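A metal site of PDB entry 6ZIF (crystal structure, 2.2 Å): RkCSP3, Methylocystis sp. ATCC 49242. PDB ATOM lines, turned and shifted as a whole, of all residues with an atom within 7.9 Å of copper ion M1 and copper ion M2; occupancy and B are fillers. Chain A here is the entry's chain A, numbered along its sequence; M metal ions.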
ATOM      1  N   CYS A  18      -8.989  24.565 -18.702  1.00  0.00           N
ATOM      2  CA  CYS A  18      -9.623  23.396 -18.111  1.00  0.00           C
ATOM      3  C   CYS A  18      -8.596  22.420 -17.534  1.00  0.00           C
ATOM      4  O   CYS A  18      -8.817  21.845 -16.470  1.00  0.00           O
ATOM      5  CB  CYS A  18     -10.514  22.721 -19.148  1.00  0.00           C
ATOM      6  SG  CYS A  18     -12.003  23.706 -19.505  1.00  0.00           S
ATOM      7  N   MET A  21      -6.710  24.315 -14.502  1.00  0.00           N
ATOM      8  CA  MET A  21      -7.596  24.441 -13.342  1.00  0.00           C
ATOM      9  C   MET A  21      -7.819  23.095 -12.668  1.00  0.00           C
ATOM     10  O   MET A  21      -7.719  22.970 -11.452  1.00  0.00           O
ATOM     11  CB  MET A  21      -8.959  25.000 -13.774  1.00  0.00           C
ATOM     12  CG  MET A  21      -8.966  26.484 -14.039  1.00  0.00           C
ATOM     13  SD  MET A  21      -8.825  27.439 -12.518  1.00  0.00           S
ATOM     14  CE  MET A  21      -7.048  27.592 -12.356  1.00  0.00           C
ATOM     15  N   ALA A  22      -8.132  22.056 -13.471  1.00  0.00           N
ATOM     16  CA  ALA A  22      -8.388  20.756 -12.892  1.00  0.00           C
ATOM     17  C   ALA A  22      -7.199  20.318 -12.040  1.00  0.00           C
ATOM     18  O   ALA A  22      -7.381  19.840 -10.921  1.00  0.00           O
ATOM     19  CB  ALA A  22      -8.699  19.758 -13.964  1.00  0.00           C
ATOM     20  N   MET A  23      -5.980  20.471 -12.563  1.00  0.00           N
ATOM     21  CA  MET A  23      -4.849  19.807 -11.931  1.00  0.00           C
ATOM     22  C   MET A  23      -4.229  20.708 -10.862  1.00  0.00           C
ATOM     23  O   MET A  23      -3.345  20.276 -10.143  1.00  0.00           O
ATOM     24  CB  MET A  23      -3.788  19.442 -12.967  1.00  0.00           C
ATOM     25  CG  MET A  23      -4.274  18.379 -13.950  1.00  0.00           C
ATOM     26  SD  MET A  23      -4.825  16.837 -13.121  1.00  0.00           S
ATOM     27  CE  MET A  23      -3.298  16.392 -12.289  1.00  0.00           C
ATOM     28  N   THR A  24      -4.681  21.962 -10.776  1.00  0.00           N
ATOM     29  CA  THR A  24      -4.179  22.863  -9.737  1.00  0.00           C
ATOM     30  C   THR A  24      -5.315  23.215  -8.780  1.00  0.00           C
ATOM     31  O   THR A  24      -5.533  22.490  -7.808  1.00  0.00           O
ATOM     32  CB  THR A  24      -3.339  24.026 -10.306  1.00  0.00           C
ATOM     33  OG1 THR A  24      -4.236  24.842 -11.042  1.00  0.00           O
ATOM     34  CG2 THR A  24      -2.207  23.539 -11.189  1.00  0.00           C
ATOM     35  N   HIS A  25      -6.077  24.270  -9.095  1.00  0.00           N
ATOM     36  CA  HIS A  25      -7.162  24.701  -8.223  1.00  0.00           C
ATOM     37  C   HIS A  25      -8.084  23.562  -7.785  1.00  0.00           C
ATOM     38  O   HIS A  25      -8.298  23.379  -6.584  1.00  0.00           O
ATOM     39  CB  HIS A  25      -7.920  25.892  -8.812  1.00  0.00           C
ATOM     40  CG  HIS A  25      -9.069  26.294  -7.940  1.00  0.00           C
ATOM     41  ND1 HIS A  25      -8.882  27.056  -6.786  1.00  0.00           N
ATOM     42  CD2 HIS A  25     -10.399  26.001  -7.986  1.00  0.00           C
ATOM     43  CE1 HIS A  25     -10.051  27.252  -6.202  1.00  0.00           C
ATOM     44  NE2 HIS A  25     -10.985  26.605  -6.911  1.00  0.00           N
ATOM     45  N   CYS A  26      -8.681  22.825  -8.727  1.00  0.00           N
ATOM     46  CA  CYS A  26      -9.682  21.816  -8.367  1.00  0.00           C
ATOM     47  C   CYS A  26      -9.073  20.696  -7.522  1.00  0.00           C
ATOM     48  O   CYS A  26      -9.627  20.305  -6.506  1.00  0.00           O
ATOM     49  CB  CYS A  26     -10.349  21.215  -9.591  1.00  0.00           C
ATOM     50  SG  CYS A  26     -11.178  22.482 -10.562  1.00  0.00           S
ATOM     51  N   LEU A  27      -7.930  20.160  -7.967  1.00  0.00           N
ATOM     52  CA  LEU A  27      -7.256  19.101  -7.226  1.00  0.00           C
ATOM     53  C   LEU A  27      -6.880  19.594  -5.827  1.00  0.00           C
ATOM     54  O   LEU A  27      -6.941  18.842  -4.868  1.00  0.00           O
ATOM     55  CB  LEU A  27      -6.011  18.642  -7.989  1.00  0.00           C
ATOM     56  CG  LEU A  27      -5.418  17.288  -7.645  1.00  0.00           C
ATOM     57  CD1 LEU A  27      -6.487  16.198  -7.671  1.00  0.00           C
ATOM     58  CD2 LEU A  27      -4.320  16.923  -8.643  1.00  0.00           C
ATOM     59  N   GLU A  28      -6.486  20.874  -5.698  1.00  0.00           N
ATOM     60  CA  GLU A  28      -6.005  21.352  -4.421  1.00  0.00           C
ATOM     61  C   GLU A  28      -7.163  21.694  -3.487  1.00  0.00           C
ATOM     62  O   GLU A  28      -7.008  21.628  -2.281  1.00  0.00           O
ATOM     63  CB  GLU A  28      -4.941  22.435  -4.553  1.00  0.00           C
ATOM     64  CG  GLU A  28      -3.581  21.797  -4.766  1.00  0.00           C
ATOM     65  CD  GLU A  28      -2.666  22.439  -5.801  1.00  0.00           C
ATOM     66  OE1 GLU A  28      -2.750  23.687  -5.986  1.00  0.00           O
ATOM     67  OE2 GLU A  28      -1.895  21.702  -6.466  1.00  0.00           O
ATOM     68  N   THR A  29      -8.312  22.064  -4.046  1.00  0.00           N
ATOM     69  CA  THR A  29      -9.474  22.381  -3.216  1.00  0.00           C
ATOM     70  C   THR A  29     -10.143  21.091  -2.749  1.00  0.00           C
ATOM     71  O   THR A  29     -10.618  21.017  -1.621  1.00  0.00           O
ATOM     72  CB  THR A  29     -10.448  23.288  -3.970  1.00  0.00           C
ATOM     73  OG1 THR A  29      -9.702  24.429  -4.374  1.00  0.00           O
ATOM     74  CG2 THR A  29     -11.606  23.735  -3.106  1.00  0.00           C
ATOM     75  N   GLY A  30     -10.241  20.077  -3.620  1.00  0.00           N
ATOM     76  CA  GLY A  30     -11.020  18.878  -3.296  1.00  0.00           C
ATOM     77  C   GLY A  30     -12.508  19.197  -3.261  1.00  0.00           C
ATOM     78  O   GLY A  30     -12.978  20.175  -3.882  1.00  0.00           O
ATOM     79  N   ASP A  32     -16.353  19.326  -3.956  1.00  0.00           N
ATOM     80  CA  ASP A  32     -17.102  19.328  -5.211  1.00  0.00           C
ATOM     81  C   ASP A  32     -16.182  19.458  -6.434  1.00  0.00           C
ATOM     82  O   ASP A  32     -16.564  19.084  -7.538  1.00  0.00           O
ATOM     83  CB  ASP A  32     -18.184  20.401  -5.199  1.00  0.00           C
ATOM     84  CG  ASP A  32     -19.186  20.224  -4.066  1.00  0.00           C
ATOM     85  OD1 ASP A  32     -19.618  19.063  -3.771  1.00  0.00           O
ATOM     86  OD2 ASP A  32     -19.553  21.255  -3.461  1.00  0.00           O
ATOM     87  N   HIS A  33     -14.984  19.990  -6.227  1.00  0.00           N
ATOM     88  CA  HIS A  33     -14.091  20.261  -7.358  1.00  0.00           C
ATOM     89  C   HIS A  33     -13.527  18.975  -7.954  1.00  0.00           C
ATOM     90  O   HIS A  33     -13.050  19.012  -9.076  1.00  0.00           O
ATOM     91  CB  HIS A  33     -12.972  21.214  -6.969  1.00  0.00           C
ATOM     92  CG  HIS A  33     -13.497  22.555  -6.601  1.00  0.00           C
ATOM     93  ND1 HIS A  33     -13.539  23.601  -7.510  1.00  0.00           N
ATOM     94  CD2 HIS A  33     -14.038  23.015  -5.443  1.00  0.00           C
ATOM     95  CE1 HIS A  33     -14.051  24.664  -6.919  1.00  0.00           C
ATOM     96  NE2 HIS A  33     -14.370  24.326  -5.647  1.00  0.00           N
ATOM     97  N   VAL A  34     -13.628  17.849  -7.233  1.00  0.00           N
ATOM     98  CA  VAL A  34     -13.075  16.595  -7.684  1.00  0.00           C
ATOM     99  C   VAL A  34     -14.160  15.521  -7.759  1.00  0.00           C
ATOM    100  O   VAL A  34     -13.830  14.357  -7.939  1.00  0.00           O
ATOM    101  CB  VAL A  34     -11.860  16.110  -6.851  1.00  0.00           C
ATOM    102  CG1 VAL A  34     -10.665  17.024  -6.977  1.00  0.00           C
ATOM    103  CG2 VAL A  34     -12.208  15.848  -5.402  1.00  0.00           C
ATOM    104  N   LYS A  35     -15.421  15.916  -7.645  1.00  0.00           N
ATOM    105  CA  LYS A  35     -16.499  14.957  -7.840  1.00  0.00           C
ATOM    106  C   LYS A  35     -16.431  14.413  -9.264  1.00  0.00           C
ATOM    107  O   LYS A  35     -16.207  15.175 -10.205  1.00  0.00           O
ATOM    108  CB  LYS A  35     -17.860  15.578  -7.498  1.00  0.00           C
ATOM    109  CG  LYS A  35     -18.227  15.464  -6.032  1.00  0.00           C
ATOM    110  CD  LYS A  35     -19.641  15.934  -5.761  1.00  0.00           C
ATOM    111  CE  LYS A  35     -19.977  15.875  -4.283  1.00  0.00           C
ATOM    112  NZ  LYS A  35     -21.261  16.560  -4.018  1.00  0.00           N
ATOM    113  N   HIS A  38     -18.101  16.313 -12.526  1.00  0.00           N
ATOM    114  CA  HIS A  38     -17.510  17.613 -12.804  1.00  0.00           C
ATOM    115  C   HIS A  38     -16.060  17.453 -13.281  1.00  0.00           C
ATOM    116  O   HIS A  38     -15.634  18.106 -14.230  1.00  0.00           O
ATOM    117  CB  HIS A  38     -17.521  18.494 -11.540  1.00  0.00           C
ATOM    118  CG  HIS A  38     -16.563  19.617 -11.611  1.00  0.00           C
ATOM    119  ND1 HIS A  38     -16.850  20.774 -12.320  1.00  0.00           N
ATOM    120  CD2 HIS A  38     -15.312  19.774 -11.115  1.00  0.00           C
ATOM    121  CE1 HIS A  38     -15.824  21.598 -12.248  1.00  0.00           C
ATOM    122  NE2 HIS A  38     -14.872  21.016 -11.502  1.00  0.00           N
ATOM    123  N   PHE A  39     -15.296  16.587 -12.623  1.00  0.00           N
ATOM    124  CA  PHE A  39     -13.873  16.536 -12.905  1.00  0.00           C
ATOM    125  C   PHE A  39     -13.621  15.870 -14.259  1.00  0.00           C
ATOM    126  O   PHE A  39     -12.780  16.315 -15.030  1.00  0.00           O
ATOM    127  CB  PHE A  39     -13.131  15.751 -11.811  1.00  0.00           C
ATOM    128  CG  PHE A  39     -11.636  15.919 -11.836  1.00  0.00           C
ATOM    129  CD1 PHE A  39     -11.036  17.018 -11.228  1.00  0.00           C
ATOM    130  CD2 PHE A  39     -10.828  15.025 -12.511  1.00  0.00           C
ATOM    131  CE1 PHE A  39      -9.657  17.146 -11.222  1.00  0.00           C
ATOM    132  CE2 PHE A  39      -9.456  15.167 -12.540  1.00  0.00           C
ATOM    133  CZ  PHE A  39      -8.872  16.231 -11.900  1.00  0.00           C
ATOM    134  N   ARG A  40     -14.399  14.820 -14.527  1.00  0.00           N
ATOM    135  CA  ARG A  40     -14.337  14.103 -15.785  1.00  0.00           C
ATOM    136  C   ARG A  40     -14.688  15.038 -16.936  1.00  0.00           C
ATOM    137  O   ARG A  40     -14.060  15.018 -17.991  1.00  0.00           O
ATOM    138  CB  ARG A  40     -15.185  12.835 -15.713  1.00  0.00           C
ATOM    139  CG  ARG A  40     -15.205  12.030 -16.999  1.00  0.00           C
ATOM    140  CD  ARG A  40     -16.044  10.780 -16.743  1.00  0.00           C
ATOM    141  NE  ARG A  40     -15.251   9.825 -15.988  1.00  0.00           N
ATOM    142  CZ  ARG A  40     -15.681   9.179 -14.918  1.00  0.00           C
ATOM    143  NH1 ARG A  40     -16.900   9.409 -14.482  1.00  0.00           N
ATOM    144  NH2 ARG A  40     -14.884   8.320 -14.299  1.00  0.00           N
ATOM    145  N   MET A  42     -14.175  18.213 -17.011  1.00  0.00           N
ATOM    146  CA  MET A  42     -13.048  19.129 -17.177  1.00  0.00           C
ATOM    147  C   MET A  42     -11.910  18.481 -17.964  1.00  0.00           C
ATOM    148  O   MET A  42     -11.377  19.099 -18.883  1.00  0.00           O
ATOM    149  CB  MET A  42     -12.535  19.650 -15.824  1.00  0.00           C
ATOM    150  CG  MET A  42     -13.446  20.742 -15.247  1.00  0.00           C
ATOM    151  SD  MET A  42     -13.132  22.393 -15.984  1.00  0.00           S
ATOM    152  CE  MET A  42     -11.686  22.861 -15.028  1.00  0.00           C
ATOM    153  N   GLU A  80     -21.268  22.145 -16.277  1.00  0.00           N
ATOM    154  CA  GLU A  80     -20.737  21.494 -15.075  1.00  0.00           C
ATOM    155  C   GLU A  80     -19.859  22.446 -14.261  1.00  0.00           C
ATOM    156  O   GLU A  80     -19.419  22.067 -13.173  1.00  0.00           O
ATOM    157  CB  GLU A  80     -19.862  20.293 -15.443  1.00  0.00           C
ATOM    158  CG  GLU A  80     -20.644  19.115 -16.000  1.00  0.00           C
ATOM    159  CD  GLU A  80     -21.585  18.531 -14.966  1.00  0.00           C
ATOM    160  OE1 GLU A  80     -21.211  18.475 -13.784  1.00  0.00           O
ATOM    161  OE2 GLU A  80     -22.705  18.123 -15.349  1.00  0.00           O
ATOM    162  N   CYS A  81     -19.580  23.647 -14.770  1.00  0.00           N
ATOM    163  CA  CYS A  81     -18.703  24.531 -14.023  1.00  0.00           C
ATOM    164  C   CYS A  81     -19.517  25.684 -13.427  1.00  0.00           C
ATOM    165  O   CYS A  81     -19.033  26.363 -12.556  1.00  0.00           O
ATOM    166  CB  CYS A  81     -17.567  25.020 -14.901  1.00  0.00           C
ATOM    167  SG  CYS A  81     -16.151  23.889 -14.965  1.00  0.00           S
ATOM    168  N   LEU A  84     -20.322  25.784  -9.474  1.00  0.00           N
ATOM    169  CA  LEU A  84     -19.281  25.729  -8.466  1.00  0.00           C
ATOM    170  C   LEU A  84     -18.703  27.113  -8.204  1.00  0.00           C
ATOM    171  O   LEU A  84     -18.410  27.885  -9.125  1.00  0.00           O
ATOM    172  CB  LEU A  84     -18.185  24.755  -8.908  1.00  0.00           C
ATOM    173  CG  LEU A  84     -18.428  23.280  -8.596  1.00  0.00           C
ATOM    174  CD1 LEU A  84     -19.505  22.695  -9.521  1.00  0.00           C
ATOM    175  CD2 LEU A  84     -17.091  22.526  -8.762  1.00  0.00           C
ATOM    176  N   PRO A  85     -18.447  27.441  -6.920  1.00  0.00           N
ATOM    177  CA  PRO A  85     -17.639  28.603  -6.553  1.00  0.00           C
ATOM    178  C   PRO A  85     -16.272  28.534  -7.216  1.00  0.00           C
ATOM    179  O   PRO A  85     -15.643  27.476  -7.280  1.00  0.00           O
ATOM    180  CB  PRO A  85     -17.443  28.408  -5.031  1.00  0.00           C
ATOM    181  CG  PRO A  85     -17.685  26.932  -4.797  1.00  0.00           C
ATOM    182  CD  PRO A  85     -18.827  26.633  -5.745  1.00  0.00           C
ATOM    183  N   ASP A  86     -15.864  29.663  -7.770  1.00  0.00           N
ATOM    184  CA  ASP A  86     -14.529  29.827  -8.329  1.00  0.00           C
ATOM    185  C   ASP A  86     -14.464  29.329  -9.769  1.00  0.00           C
ATOM    186  O   ASP A  86     -13.425  29.536 -10.384  1.00  0.00           O
ATOM    187  CB  ASP A  86     -13.432  29.194  -7.463  1.00  0.00           C
ATOM    188  CG  ASP A  86     -13.255  29.893  -6.115  1.00  0.00           C
ATOM    189  OD1 ASP A  86     -13.405  31.133  -6.054  1.00  0.00           O
ATOM    190  OD2 ASP A  86     -12.942  29.184  -5.140  1.00  0.00           O
ATOM    191  N   MET A  87     -15.546  28.725 -10.303  1.00  0.00           N
ATOM    192  CA  MET A  87     -15.412  28.111 -11.621  1.00  0.00           C
ATOM    193  C   MET A  87     -16.113  28.931 -12.713  1.00  0.00           C
ATOM    194  O   MET A  87     -16.293  28.450 -13.826  1.00  0.00           O
ATOM    195  CB  MET A  87     -15.980  26.692 -11.641  1.00  0.00           C
ATOM    196  CG  MET A  87     -15.408  25.762 -10.613  1.00  0.00           C
ATOM    197  SD  MET A  87     -13.618  25.525 -10.801  1.00  0.00           S
ATOM    198  CE  MET A  87     -13.551  24.646 -12.361  1.00  0.00           C
ATOM    199  N   CYS A  90     -13.923  29.772 -15.743  1.00  0.00           N
ATOM    200  CA  CYS A  90     -13.719  28.597 -16.576  1.00  0.00           C
ATOM    201  C   CYS A  90     -14.950  28.408 -17.456  1.00  0.00           C
ATOM    202  O   CYS A  90     -14.809  28.230 -18.685  1.00  0.00           O
ATOM    203  CB  CYS A  90     -13.479  27.346 -15.739  1.00  0.00           C
ATOM    204  SG  CYS A  90     -13.086  25.884 -16.749  1.00  0.00           S
HETATM  205 CU    CU M   1     -12.726  23.791  -9.508  1.00  0.00          CU
HETATM  206 CU    CU M   2     -13.119  21.627 -11.006  1.00  0.00          CU
HETATM  207 CU    CU M   3     -14.466  24.393 -16.119  1.00  0.00          CU
HETATM  208 CU    CU M   4     -16.416  22.830 -16.944  1.00  0.00          CU
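Copper ion M2 is bound by a ring nitrogen (NE2) of His 38 (1.9 Å) and the side-chain sulfur of Cys 26 (2.2 Å).
The nearest printed residue that does not touch copper ion M2 is Met 42 (4.3 Å).
Copper ion M1 is bound by ND1 of His 33, SG of Cys 26 and SD of Met 87.
O of His 25 lies within hydrogen-bond range of OG1 of Thr 29, 2.8 Å away. The backbone NH of Cys 26 is in hydrogen-bond range of the backbone carbonyl oxygen of Met 21 (2.9 Å). A ring nitrogen (ND1) of His 38 sits at hydrogen-bond distance from the backbone carbonyl oxygen (O) of Glu 80 (3.0 Å).
Residues that only touch copper ion M1: His 25. Within 4 Å of copper ion M1: His 25, Cys 26, His 33 and Met 87. Along chain A the residues within 4 Å of copper ion M1 span positions 25 to 87. The nearest printed residue that does not touch copper ion M1 is His 38 (4.04 Å).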
